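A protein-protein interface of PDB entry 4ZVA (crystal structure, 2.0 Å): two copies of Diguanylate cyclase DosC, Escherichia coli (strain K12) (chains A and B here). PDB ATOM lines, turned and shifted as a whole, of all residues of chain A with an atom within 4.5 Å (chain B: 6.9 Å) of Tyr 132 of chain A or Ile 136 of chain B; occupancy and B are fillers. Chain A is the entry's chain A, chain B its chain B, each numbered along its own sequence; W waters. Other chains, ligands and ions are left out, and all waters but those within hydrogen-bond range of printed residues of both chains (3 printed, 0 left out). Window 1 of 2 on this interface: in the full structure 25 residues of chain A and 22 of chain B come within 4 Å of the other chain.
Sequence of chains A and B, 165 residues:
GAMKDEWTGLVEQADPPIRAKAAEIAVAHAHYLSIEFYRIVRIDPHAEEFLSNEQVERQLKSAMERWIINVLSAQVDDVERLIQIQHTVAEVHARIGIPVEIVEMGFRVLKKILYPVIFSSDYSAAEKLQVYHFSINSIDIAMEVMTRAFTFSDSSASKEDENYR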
ATOM      1  N   TYR A 115      -9.479  23.107   9.675  1.00  0.00           N
ATOM      2  CA  TYR A 115     -10.105  21.922   9.089  1.00  0.00           C
ATOM      3  C   TYR A 115     -11.406  22.221   8.325  1.00  0.00           C
ATOM      4  O   TYR A 115     -11.544  21.780   7.185  1.00  0.00           O
ATOM      5  CB  TYR A 115     -10.369  20.860  10.165  1.00  0.00           C
ATOM      6  CG  TYR A 115     -11.094  19.640   9.639  1.00  0.00           C
ATOM      7  CD1 TYR A 115     -10.411  18.643   8.958  1.00  0.00           C
ATOM      8  CD2 TYR A 115     -12.463  19.485   9.827  1.00  0.00           C
ATOM      9  CE1 TYR A 115     -11.068  17.528   8.474  1.00  0.00           C
ATOM     10  CE2 TYR A 115     -13.129  18.371   9.347  1.00  0.00           C
ATOM     11  CZ  TYR A 115     -12.424  17.396   8.674  1.00  0.00           C
ATOM     12  OH  TYR A 115     -13.081  16.283   8.195  1.00  0.00           O
ATOM     13  N   ILE A 118     -10.659  23.615   4.935  1.00  0.00           N
ATOM     14  CA  ILE A 118     -10.183  22.612   3.989  1.00  0.00           C
ATOM     15  C   ILE A 118     -11.315  21.669   3.589  1.00  0.00           C
ATOM     16  O   ILE A 118     -11.440  21.283   2.425  1.00  0.00           O
ATOM     17  CB  ILE A 118      -9.005  21.802   4.578  1.00  0.00           C
ATOM     18  CG1 ILE A 118      -7.810  22.725   4.827  1.00  0.00           C
ATOM     19  CG2 ILE A 118      -8.606  20.665   3.649  1.00  0.00           C
ATOM     20  CD1 ILE A 118      -6.590  22.024   5.395  1.00  0.00           C
ATOM     21  N   LYS A 128      -8.057  16.553   0.108  1.00  0.00           N
ATOM     22  CA  LYS A 128      -8.318  17.197   1.392  1.00  0.00           C
ATOM     23  C   LYS A 128      -7.512  16.550   2.515  1.00  0.00           C
ATOM     24  O   LYS A 128      -6.957  17.239   3.364  1.00  0.00           O
ATOM     25  CB  LYS A 128      -9.808  17.144   1.726  1.00  0.00           C
ATOM     26  CG  LYS A 128     -10.689  18.005   0.828  1.00  0.00           C
ATOM     27  CD  LYS A 128     -12.157  17.821   1.177  1.00  0.00           C
ATOM     28  CE  LYS A 128     -13.050  18.705   0.319  1.00  0.00           C
ATOM     29  NZ  LYS A 128     -14.491  18.453   0.588  1.00  0.00           N
ATOM     30  N   LEU A 129      -7.455  15.223   2.508  1.00  0.00           N
ATOM     31  CA  LEU A 129      -6.711  14.475   3.519  1.00  0.00           C
ATOM     32  C   LEU A 129      -5.228  14.828   3.503  1.00  0.00           C
ATOM     33  O   LEU A 129      -4.624  15.077   4.546  1.00  0.00           O
ATOM     34  CB  LEU A 129      -6.883  12.971   3.303  1.00  0.00           C
ATOM     35  CG  LEU A 129      -6.051  12.060   4.213  1.00  0.00           C
ATOM     36  CD1 LEU A 129      -6.464  12.223   5.668  1.00  0.00           C
ATOM     37  CD2 LEU A 129      -6.156  10.605   3.771  1.00  0.00           C
ATOM     38  N   GLN A 130      -4.645  14.842   2.309  1.00  0.00           N
ATOM     39  CA  GLN A 130      -3.225  15.119   2.159  1.00  0.00           C
ATOM     40  C   GLN A 130      -2.888  16.583   2.428  1.00  0.00           C
ATOM     41  O   GLN A 130      -1.832  16.891   2.982  1.00  0.00           O
ATOM     42  CB  GLN A 130      -2.763  14.711   0.762  1.00  0.00           C
ATOM     43  CG  GLN A 130      -2.822  13.210   0.541  1.00  0.00           C
ATOM     44  CD  GLN A 130      -2.199  12.787  -0.769  1.00  0.00           C
ATOM     45  OE1 GLN A 130      -2.731  13.068  -1.842  1.00  0.00           O
ATOM     46  NE2 GLN A 130      -1.061  12.104  -0.689  1.00  0.00           N
ATOM     47  N   VAL A 131      -3.784  17.485   2.039  1.00  0.00           N
ATOM     48  CA  VAL A 131      -3.585  18.903   2.301  1.00  0.00           C
ATOM     49  C   VAL A 131      -3.669  19.176   3.798  1.00  0.00           C
ATOM     50  O   VAL A 131      -2.862  19.919   4.354  1.00  0.00           O
ATOM     51  CB  VAL A 131      -4.617  19.773   1.549  1.00  0.00           C
ATOM     52  CG1 VAL A 131      -4.599  21.197   2.071  1.00  0.00           C
ATOM     53  CG2 VAL A 131      -4.335  19.747   0.057  1.00  0.00           C
ATOM     54  N   TYR A 132      -4.655  18.565   4.445  1.00  0.00           N
ATOM     55  CA  TYR A 132      -4.838  18.715   5.881  1.00  0.00           C
ATOM     56  C   TYR A 132      -3.646  18.130   6.642  1.00  0.00           C
ATOM     57  O   TYR A 132      -3.183  18.712   7.621  1.00  0.00           O
ATOM     58  CB  TYR A 132      -6.143  18.044   6.311  1.00  0.00           C
ATOM     59  CG  TYR A 132      -6.424  18.072   7.793  1.00  0.00           C
ATOM     60  CD1 TYR A 132      -6.617  19.271   8.463  1.00  0.00           C
ATOM     61  CD2 TYR A 132      -6.525  16.892   8.518  1.00  0.00           C
ATOM     62  CE1 TYR A 132      -6.887  19.297   9.821  1.00  0.00           C
ATOM     63  CE2 TYR A 132      -6.795  16.905   9.870  1.00  0.00           C
ATOM     64  CZ  TYR A 132      -6.974  18.107  10.518  1.00  0.00           C
ATOM     65  OH  TYR A 132      -7.242  18.113  11.868  1.00  0.00           O
ATOM     66  N   HIS A 133      -3.147  16.989   6.176  1.00  0.00           N
ATOM     67  CA  HIS A 133      -1.980  16.353   6.791  1.00  0.00           C
ATOM     68  C   HIS A 133      -0.736  17.233   6.710  1.00  0.00           C
ATOM     69  O   HIS A 133      -0.082  17.486   7.722  1.00  0.00           O
ATOM     70  CB  HIS A 133      -1.697  15.005   6.129  1.00  0.00           C
ATOM     71  CG  HIS A 133      -0.385  14.399   6.527  1.00  0.00           C
ATOM     72  ND1 HIS A 133       0.649  14.214   5.638  1.00  0.00           N
ATOM     73  CD2 HIS A 133       0.061  13.950   7.725  1.00  0.00           C
ATOM     74  CE1 HIS A 133       1.676  13.667   6.267  1.00  0.00           C
ATOM     75  NE2 HIS A 133       1.345  13.498   7.533  1.00  0.00           N
ATOM     76  N   PHE A 134      -0.416  17.696   5.505  1.00  0.00           N
ATOM     77  CA  PHE A 134       0.718  18.594   5.308  1.00  0.00           C
ATOM     78  C   PHE A 134       0.592  19.834   6.182  1.00  0.00           C
ATOM     79  O   PHE A 134       1.569  20.282   6.783  1.00  0.00           O
ATOM     80  CB  PHE A 134       0.840  19.001   3.836  1.00  0.00           C
ATOM     81  CG  PHE A 134       1.934  19.998   3.574  1.00  0.00           C
ATOM     82  CD1 PHE A 134       3.252  19.585   3.472  1.00  0.00           C
ATOM     83  CD2 PHE A 134       1.647  21.346   3.430  1.00  0.00           C
ATOM     84  CE1 PHE A 134       4.264  20.496   3.234  1.00  0.00           C
ATOM     85  CE2 PHE A 134       2.654  22.263   3.192  1.00  0.00           C
ATOM     86  CZ  PHE A 134       3.965  21.837   3.093  1.00  0.00           C
ATOM     87  N   SER A 135      -0.620  20.374   6.256  1.00  0.00           N
ATOM     88  CA  SER A 135      -0.888  21.573   7.039  1.00  0.00           C
ATOM     89  C   SER A 135      -0.690  21.325   8.532  1.00  0.00           C
ATOM     90  O   SER A 135      -0.079  22.136   9.220  1.00  0.00           O
ATOM     91  CB  SER A 135      -2.309  22.075   6.779  1.00  0.00           C
ATOM     92  OG  SER A 135      -2.481  22.443   5.418  1.00  0.00           O
ATOM     93  N   ILE A 136      -1.220  20.212   9.032  1.00  0.00           N
ATOM     94  CA  ILE A 136      -1.073  19.878  10.446  1.00  0.00           C
ATOM     95  C   ILE A 136       0.401  19.695  10.805  1.00  0.00           C
ATOM     96  O   ILE A 136       0.884  20.263  11.783  1.00  0.00           O
ATOM     97  CB  ILE A 136      -1.852  18.602  10.822  1.00  0.00           C
ATOM     98  CG1 ILE A 136      -3.359  18.859  10.760  1.00  0.00           C
ATOM     99  CG2 ILE A 136      -1.475  18.138  12.221  1.00  0.00           C
ATOM    100  CD1 ILE A 136      -3.833  19.958  11.695  1.00  0.00           C
ATOM    101  N   LEU B  10     -16.542  17.136  21.185  1.00  0.00           N
ATOM    102  CA  LEU B  10     -15.817  16.500  20.087  1.00  0.00           C
ATOM    103  C   LEU B  10     -16.225  15.037  19.916  1.00  0.00           C
ATOM    104  O   LEU B  10     -16.425  14.565  18.797  1.00  0.00           O
ATOM    105  CB  LEU B  10     -14.308  16.598  20.314  1.00  0.00           C
ATOM    106  CG  LEU B  10     -13.415  15.910  19.278  1.00  0.00           C
ATOM    107  CD1 LEU B  10     -13.562  16.572  17.915  1.00  0.00           C
ATOM    108  CD2 LEU B  10     -11.958  15.902  19.723  1.00  0.00           C
ATOM    109  N   LEU B  72      -8.089   7.744  21.676  1.00  0.00           N
ATOM    110  CA  LEU B  72      -8.760   7.601  20.385  1.00  0.00           C
ATOM    111  C   LEU B  72     -10.051   6.780  20.448  1.00  0.00           C
ATOM    112  O   LEU B  72     -10.899   6.896  19.561  1.00  0.00           O
ATOM    113  CB  LEU B  72      -7.802   6.980  19.366  1.00  0.00           C
ATOM    114  CG  LEU B  72      -6.574   7.829  19.024  1.00  0.00           C
ATOM    115  CD1 LEU B  72      -5.759   7.190  17.912  1.00  0.00           C
ATOM    116  CD2 LEU B  72      -6.986   9.242  18.645  1.00  0.00           C
ATOM    117  N   LEU B 110       4.042  11.536  17.666  1.00  0.00           N
ATOM    118  CA  LEU B 110       2.870  10.664  17.681  1.00  0.00           C
ATOM    119  C   LEU B 110       1.894  10.998  16.555  1.00  0.00           C
ATOM    120  O   LEU B 110       1.467  10.118  15.810  1.00  0.00           O
ATOM    121  CB  LEU B 110       2.149  10.756  19.028  1.00  0.00           C
ATOM    122  CG  LEU B 110       0.863   9.933  19.147  1.00  0.00           C
ATOM    123  CD1 LEU B 110       1.144   8.450  18.921  1.00  0.00           C
ATOM    124  CD2 LEU B 110       0.204  10.161  20.494  1.00  0.00           C
ATOM    125  N   LYS B 111       1.550  12.275  16.436  1.00  0.00           N
ATOM    126  CA  LYS B 111       0.644  12.716  15.382  1.00  0.00           C
ATOM    127  C   LYS B 111       1.244  12.427  14.015  1.00  0.00           C
ATOM    128  O   LYS B 111       0.530  12.081  13.076  1.00  0.00           O
ATOM    129  CB  LYS B 111       0.327  14.205  15.536  1.00  0.00           C
ATOM    130  CG  LYS B 111      -0.575  14.500  16.722  1.00  0.00           C
ATOM    131  CD  LYS B 111      -0.818  15.988  16.901  1.00  0.00           C
ATOM    132  CE  LYS B 111       0.428  16.695  17.399  1.00  0.00           C
ATOM    133  NZ  LYS B 111       0.152  18.123  17.717  1.00  0.00           N
ATOM    134  N   LYS B 112       2.565  12.539  13.915  1.00  0.00           N
ATOM    135  CA  LYS B 112       3.252  12.284  12.653  1.00  0.00           C
ATOM    136  C   LYS B 112       3.165  10.822  12.227  1.00  0.00           C
ATOM    137  O   LYS B 112       2.823  10.527  11.082  1.00  0.00           O
ATOM    138  CB  LYS B 112       4.719  12.707  12.750  1.00  0.00           C
ATOM    139  CG  LYS B 112       5.533  12.391  11.504  1.00  0.00           C
ATOM    140  CD  LYS B 112       6.990  12.795  11.668  1.00  0.00           C
ATOM    141  CE  LYS B 112       7.825  12.342  10.480  1.00  0.00           C
ATOM    142  NZ  LYS B 112       9.247  12.763  10.601  1.00  0.00           N
ATOM    143  N   LEU B 114       1.111   8.569  13.277  1.00  0.00           N
ATOM    144  CA  LEU B 114      -0.263   8.085  13.244  1.00  0.00           C
ATOM    145  C   LEU B 114      -0.841   8.135  11.830  1.00  0.00           C
ATOM    146  O   LEU B 114      -1.606   7.257  11.430  1.00  0.00           O
ATOM    147  CB  LEU B 114      -1.137   8.902  14.195  1.00  0.00           C
ATOM    148  CG  LEU B 114      -2.633   8.588  14.220  1.00  0.00           C
ATOM    149  CD1 LEU B 114      -2.886   7.142  14.628  1.00  0.00           C
ATOM    150  CD2 LEU B 114      -3.345   9.540  15.160  1.00  0.00           C
ATOM    151  N   TYR B 115      -0.465   9.159  11.073  1.00  0.00           N
ATOM    152  CA  TYR B 115      -1.038   9.375   9.745  1.00  0.00           C
ATOM    153  C   TYR B 115      -0.810   8.235   8.738  1.00  0.00           C
ATOM    154  O   TYR B 115      -1.770   7.799   8.103  1.00  0.00           O
ATOM    155  CB  TYR B 115      -0.523  10.695   9.154  1.00  0.00           C
ATOM    156  CG  TYR B 115      -1.006  10.954   7.745  1.00  0.00           C
ATOM    157  CD1 TYR B 115      -2.281  11.450   7.509  1.00  0.00           C
ATOM    158  CD2 TYR B 115      -0.182  10.717   6.652  1.00  0.00           C
ATOM    159  CE1 TYR B 115      -2.728  11.691   6.222  1.00  0.00           C
ATOM    160  CE2 TYR B 115      -0.618  10.958   5.362  1.00  0.00           C
ATOM    161  CZ  TYR B 115      -1.890  11.446   5.153  1.00  0.00           C
ATOM    162  OH  TYR B 115      -2.328  11.687   3.872  1.00  0.00           O
ATOM    163  N   ILE B 118      -3.279   5.508   9.215  1.00  0.00           N
ATOM    164  CA  ILE B 118      -4.623   5.804   8.734  1.00  0.00           C
ATOM    165  C   ILE B 118      -4.642   5.818   7.205  1.00  0.00           C
ATOM    166  O   ILE B 118      -5.578   5.322   6.580  1.00  0.00           O
ATOM    167  CB  ILE B 118      -5.133   7.148   9.290  1.00  0.00           C
ATOM    168  CG1 ILE B 118      -5.227   7.074  10.817  1.00  0.00           C
ATOM    169  CG2 ILE B 118      -6.487   7.513   8.681  1.00  0.00           C
ATOM    170  CD1 ILE B 118      -5.729   8.341  11.476  1.00  0.00           C
ATOM    171  N   LEU B 129     -10.105  10.959   6.275  1.00  0.00           N
ATOM    172  CA  LEU B 129     -10.032  12.364   6.657  1.00  0.00           C
ATOM    173  C   LEU B 129     -10.695  12.617   8.003  1.00  0.00           C
ATOM    174  O   LEU B 129     -10.122  13.277   8.868  1.00  0.00           O
ATOM    175  CB  LEU B 129     -10.671  13.250   5.583  1.00  0.00           C
ATOM    176  CG  LEU B 129     -10.736  14.734   5.951  1.00  0.00           C
ATOM    177  CD1 LEU B 129      -9.329  15.287   6.114  1.00  0.00           C
ATOM    178  CD2 LEU B 129     -11.510  15.526   4.907  1.00  0.00           C
ATOM    179  N   VAL B 131     -11.461  10.420  10.369  1.00  0.00           N
ATOM    180  CA  VAL B 131     -10.786   9.672  11.426  1.00  0.00           C
ATOM    181  C   VAL B 131      -9.505  10.378  11.857  1.00  0.00           C
ATOM    182  O   VAL B 131      -9.229  10.519  13.050  1.00  0.00           O
ATOM    183  CB  VAL B 131     -10.456   8.239  10.972  1.00  0.00           C
ATOM    184  CG1 VAL B 131      -9.487   7.572  11.949  1.00  0.00           C
ATOM    185  CG2 VAL B 131     -11.734   7.422  10.840  1.00  0.00           C
ATOM    186  N   TYR B 132      -8.731  10.827  10.875  1.00  0.00           N
ATOM    187  CA  TYR B 132      -7.495  11.555  11.136  1.00  0.00           C
ATOM    188  C   TYR B 132      -7.787  12.881  11.839  1.00  0.00           C
ATOM    189  O   TYR B 132      -7.085  13.264  12.773  1.00  0.00           O
ATOM    190  CB  TYR B 132      -6.737  11.773   9.823  1.00  0.00           C
ATOM    191  CG  TYR B 132      -5.469  12.589   9.934  1.00  0.00           C
ATOM    192  CD1 TYR B 132      -4.393  12.145  10.689  1.00  0.00           C
ATOM    193  CD2 TYR B 132      -5.338  13.791   9.248  1.00  0.00           C
ATOM    194  CE1 TYR B 132      -3.227  12.890  10.781  1.00  0.00           C
ATOM    195  CE2 TYR B 132      -4.180  14.540   9.330  1.00  0.00           C
ATOM    196  CZ  TYR B 132      -3.128  14.087  10.098  1.00  0.00           C
ATOM    197  OH  TYR B 132      -1.975  14.837  10.178  1.00  0.00           O
ATOM    198  N   HIS B 133      -8.843  13.564  11.406  1.00  0.00           N
ATOM    199  CA  HIS B 133      -9.257  14.818  12.035  1.00  0.00           C
ATOM    200  C   HIS B 133      -9.648  14.601  13.493  1.00  0.00           C
ATOM    201  O   HIS B 133      -9.193  15.320  14.382  1.00  0.00           O
ATOM    202  CB  HIS B 133     -10.428  15.450  11.281  1.00  0.00           C
ATOM    203  CG  HIS B 133     -11.045  16.609  11.998  1.00  0.00           C
ATOM    204  ND1 HIS B 133     -12.328  16.577  12.499  1.00  0.00           N
ATOM    205  CD2 HIS B 133     -10.553  17.834  12.301  1.00  0.00           C
ATOM    206  CE1 HIS B 133     -12.601  17.733  13.077  1.00  0.00           C
ATOM    207  NE2 HIS B 133     -11.541  18.514  12.969  1.00  0.00           N
ATOM    208  N   PHE B 134     -10.516  13.623  13.727  1.00  0.00           N
ATOM    209  CA  PHE B 134     -10.912  13.259  15.084  1.00  0.00           C
ATOM    210  C   PHE B 134      -9.691  12.922  15.940  1.00  0.00           C
ATOM    211  O   PHE B 134      -9.600  13.327  17.100  1.00  0.00           O
ATOM    212  CB  PHE B 134     -11.882  12.073  15.063  1.00  0.00           C
ATOM    213  CG  PHE B 134     -12.252  11.566  16.430  1.00  0.00           C
ATOM    214  CD1 PHE B 134     -13.220  12.207  17.183  1.00  0.00           C
ATOM    215  CD2 PHE B 134     -11.624  10.451  16.965  1.00  0.00           C
ATOM    216  CE1 PHE B 134     -13.562  11.744  18.442  1.00  0.00           C
ATOM    217  CE2 PHE B 134     -11.960   9.982  18.225  1.00  0.00           C
ATOM    218  CZ  PHE B 134     -12.928  10.630  18.963  1.00  0.00           C
ATOM    219  N   SER B 135      -8.752  12.187  15.357  1.00  0.00           N
ATOM    220  CA  SER B 135      -7.550  11.776  16.075  1.00  0.00           C
ATOM    221  C   SER B 135      -6.656  12.961  16.440  1.00  0.00           C
ATOM    222  O   SER B 135      -6.195  13.064  17.573  1.00  0.00           O
ATOM    223  CB  SER B 135      -6.767  10.753  15.251  1.00  0.00           C
ATOM    224  OG  SER B 135      -7.528   9.568  15.054  1.00  0.00           O
ATOM    225  N   ILE B 136      -6.422  13.856  15.483  1.00  0.00           N
ATOM    226  CA  ILE B 136      -5.589  15.031  15.726  1.00  0.00           C
ATOM    227  C   ILE B 136      -6.181  15.929  16.808  1.00  0.00           C
ATOM    228  O   ILE B 136      -5.486  16.318  17.751  1.00  0.00           O
ATOM    229  CB  ILE B 136      -5.387  15.867  14.436  1.00  0.00           C
ATOM    230  CG1 ILE B 136      -4.529  15.104  13.427  1.00  0.00           C
ATOM    231  CG2 ILE B 136      -4.741  17.204  14.754  1.00  0.00           C
ATOM    232  CD1 ILE B 136      -3.144  14.743  13.939  1.00  0.00           C
ATOM    233  N   ASN B 137      -7.467  16.249  16.679  1.00  0.00           N
ATOM    234  CA  ASN B 137      -8.131  17.106  17.652  1.00  0.00           C
ATOM    235  C   ASN B 137      -8.167  16.467  19.039  1.00  0.00           C
ATOM    236  O   ASN B 137      -8.028  17.161  20.043  1.00  0.00           O
ATOM    237  CB  ASN B 137      -9.552  17.456  17.200  1.00  0.00           C
ATOM    238  CG  ASN B 137      -9.584  18.571  16.165  1.00  0.00           C
ATOM    239  OD1 ASN B 137      -8.564  18.911  15.562  1.00  0.00           O
ATOM    240  ND2 ASN B 137     -10.757  19.157  15.971  1.00  0.00           N
ATOM    241  N   SER B 138      -8.337  15.148  19.091  1.00  0.00           N
ATOM    242  CA  SER B 138      -8.343  14.432  20.366  1.00  0.00           C
ATOM    243  C   SER B 138      -6.983  14.501  21.049  1.00  0.00           C
ATOM    244  O   SER B 138      -6.892  14.758  22.250  1.00  0.00           O
ATOM    245  CB  SER B 138      -8.737  12.962  20.166  1.00  0.00           C
ATOM    246  OG  SER B 138     -10.082  12.838  19.738  1.00  0.00           O
ATOM    247  N   ILE B 139      -5.929  14.279  20.272  1.00  0.00           N
ATOM    248  CA  ILE B 139      -4.567  14.298  20.790  1.00  0.00           C
ATOM    249  C   ILE B 139      -4.166  15.704  21.233  1.00  0.00           C
ATOM    250  O   ILE B 139      -3.542  15.881  22.280  1.00  0.00           O
ATOM    251  CB  ILE B 139      -3.573  13.765  19.741  1.00  0.00           C
ATOM    252  CG1 ILE B 139      -3.826  12.272  19.503  1.00  0.00           C
ATOM    253  CG2 ILE B 139      -2.138  13.985  20.190  1.00  0.00           C
ATOM    254  CD1 ILE B 139      -2.922  11.642  18.471  1.00  0.00           C
ATOM    255  N   ASP B 140      -4.539  16.706  20.441  1.00  0.00           N
ATOM    256  CA  ASP B 140      -4.235  18.095  20.773  1.00  0.00           C
ATOM    257  C   ASP B 140      -4.978  18.541  22.024  1.00  0.00           C
ATOM    258  O   ASP B 140      -4.429  19.265  22.852  1.00  0.00           O
ATOM    259  CB  ASP B 140      -4.574  19.027  19.609  1.00  0.00           C
ATOM    260  CG  ASP B 140      -3.476  19.077  18.570  1.00  0.00           C
ATOM    261  OD1 ASP B 140      -2.362  18.587  18.858  1.00  0.00           O
ATOM    262  OD2 ASP B 140      -3.719  19.621  17.473  1.00  0.00           O
ATOM    263  N   ILE B 141      -6.235  18.126  22.146  1.00  0.00           N
ATOM    264  CA  ILE B 141      -7.023  18.464  23.324  1.00  0.00           C
ATOM    265  C   ILE B 141      -6.404  17.821  24.560  1.00  0.00           C
ATOM    266  O   ILE B 141      -6.310  18.445  25.618  1.00  0.00           O
ATOM    267  CB  ILE B 141      -8.492  18.005  23.175  1.00  0.00           C
ATOM    268  CG1 ILE B 141      -9.265  18.976  22.284  1.00  0.00           C
ATOM    269  CG2 ILE B 141      -9.172  17.905  24.528  1.00  0.00           C
ATOM    270  CD1 ILE B 141     -10.679  18.529  21.988  1.00  0.00           C
ATOM    271  N   ALA B 142      -5.929  16.590  24.405  1.00  0.00           N
ATOM    272  CA  ALA B 142      -5.287  15.885  25.507  1.00  0.00           C
ATOM    273  C   ALA B 142      -3.970  16.559  25.868  1.00  0.00           C
ATOM    274  O   ALA B 142      -3.631  16.682  27.043  1.00  0.00           O
ATOM    275  CB  ALA B 142      -5.059  14.426  25.151  1.00  0.00           C
HETATM  276  O   HOH W   1      -8.116  20.152  13.154  1.00  0.00           O
HETATM  277  O   HOH W   2      -0.288  11.589   2.051  1.00  0.00           O
HETATM  278  O   HOH W   3       3.063  12.059   8.962  1.00  0.00           O
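Of the 11 printed residues of chain A, 7 touch a printed residue of chain B.
Of the 21 printed residues of chain B, 5 touch a printed residue of chain A.
Among the printed residues, 12 pairs touch across the chains.
Printed residues of chain B within 4 Å of Tyr 132 of chain A: Tyr 132 (3.4 Å), His 133 (3.4 Å) and Ile 136 (3.9 Å).
Ile 136 of chain B touches just one residue of chain A: Tyr 132 (3.9 Å).
Of the printed residues of chain B, His 133 of chain A touches Tyr 115 (3.2 Å) and Tyr 132 (3.3 Å).
Of the printed residues of chain A, His 133 of chain B touches Tyr 115 and Tyr 132.
Of the printed residues of chain B, Gln 130 of chain A touches Tyr 115 (3.7 Å).
Of the printed residues of chain A, Leu 129 of chain B touches Tyr 115 (3.6 Å), Lys 128 (3.95 Å) and Leu 129 (3.7 Å).
The nearest printed residue of chain B that does not touch Tyr 132 of chain A is Asn 137 of chain B (4.004 Å).
The nearest residue of chain A that does not touch Ile 136 of chain B is Ile 136 of chain A (4.2 Å).
Tyr 115 of chain A touches Leu 129 of chain B, and with the chains exchanged Leu 129 of chain A touches Tyr 115 of chain B.
Tyr 115 of chain A touches His 133 of chain B, and with the chains exchanged His 133 of chain A touches Tyr 115 of chain B.
Tyr 132 of chain A touches His 133 of chain B, and with the chains exchanged His 133 of chain A touches Tyr 132 of chain B.
Tyr 132 of chain A touches Ile 136 of chain B, and with the chains exchanged Ile 136 of chain A touches Tyr 132 of chain B.
Of the 12 pairs that touch across the chains among the printed residues, 10 have their exchanged pair printed and touching as well.
Water W1 bridges the side-chain hydroxyl of Tyr 132 of chain A (2.6 Å) and the side-chain amide oxygen of Asn 137 of chain B (2.7 Å).
Water W3 lies within hydrogen-bond range of the backbone carbonyl oxygen of Lys 112 of chain B (2.6 Å) and a ring nitrogen (NE2) of His 133 of chain A (2.7 Å).
Water W2 lies within hydrogen-bond range of OH of Tyr 115 of chain B (2.7 Å) and NE2 of Gln 130 of chain A (2.9 Å).
The side-chain amide nitrogen (ND2) of Asn 137 of chain B lies within hydrogen-bond range of a ring nitrogen (NE2) of His 133 of chain B, 3.2 Å away.
Leu 129 of chain B touches Tyr 115 of chain A.
Tyr 115 of chain A touches His 133 of chain B (CG to CD2, 3.3 Å).
Leu 129 of chain B touches Lys 128 of chain A.
Tyr 115 of chain B touches Leu 129 of chain A.
Leu 129 of chain A touches Leu 129 of chain B.
Gln 130 of chain A touches Tyr 115 of chain B (CG to OH, 3.7 Å).
Tyr 132 of chain A touches Ile 136 of chain B (OH to CB, 3.9 Å).
His 133 of chain A touches Tyr 115 of chain B (CD2 to CG, 3.2 Å).
CD2 of His 133 of chain A touches OH of Tyr 132 of chain B, 3.3 Å away.
Tyr 132 of chain B touches Ile 136 of chain A (OH to CB, 3.8 Å).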
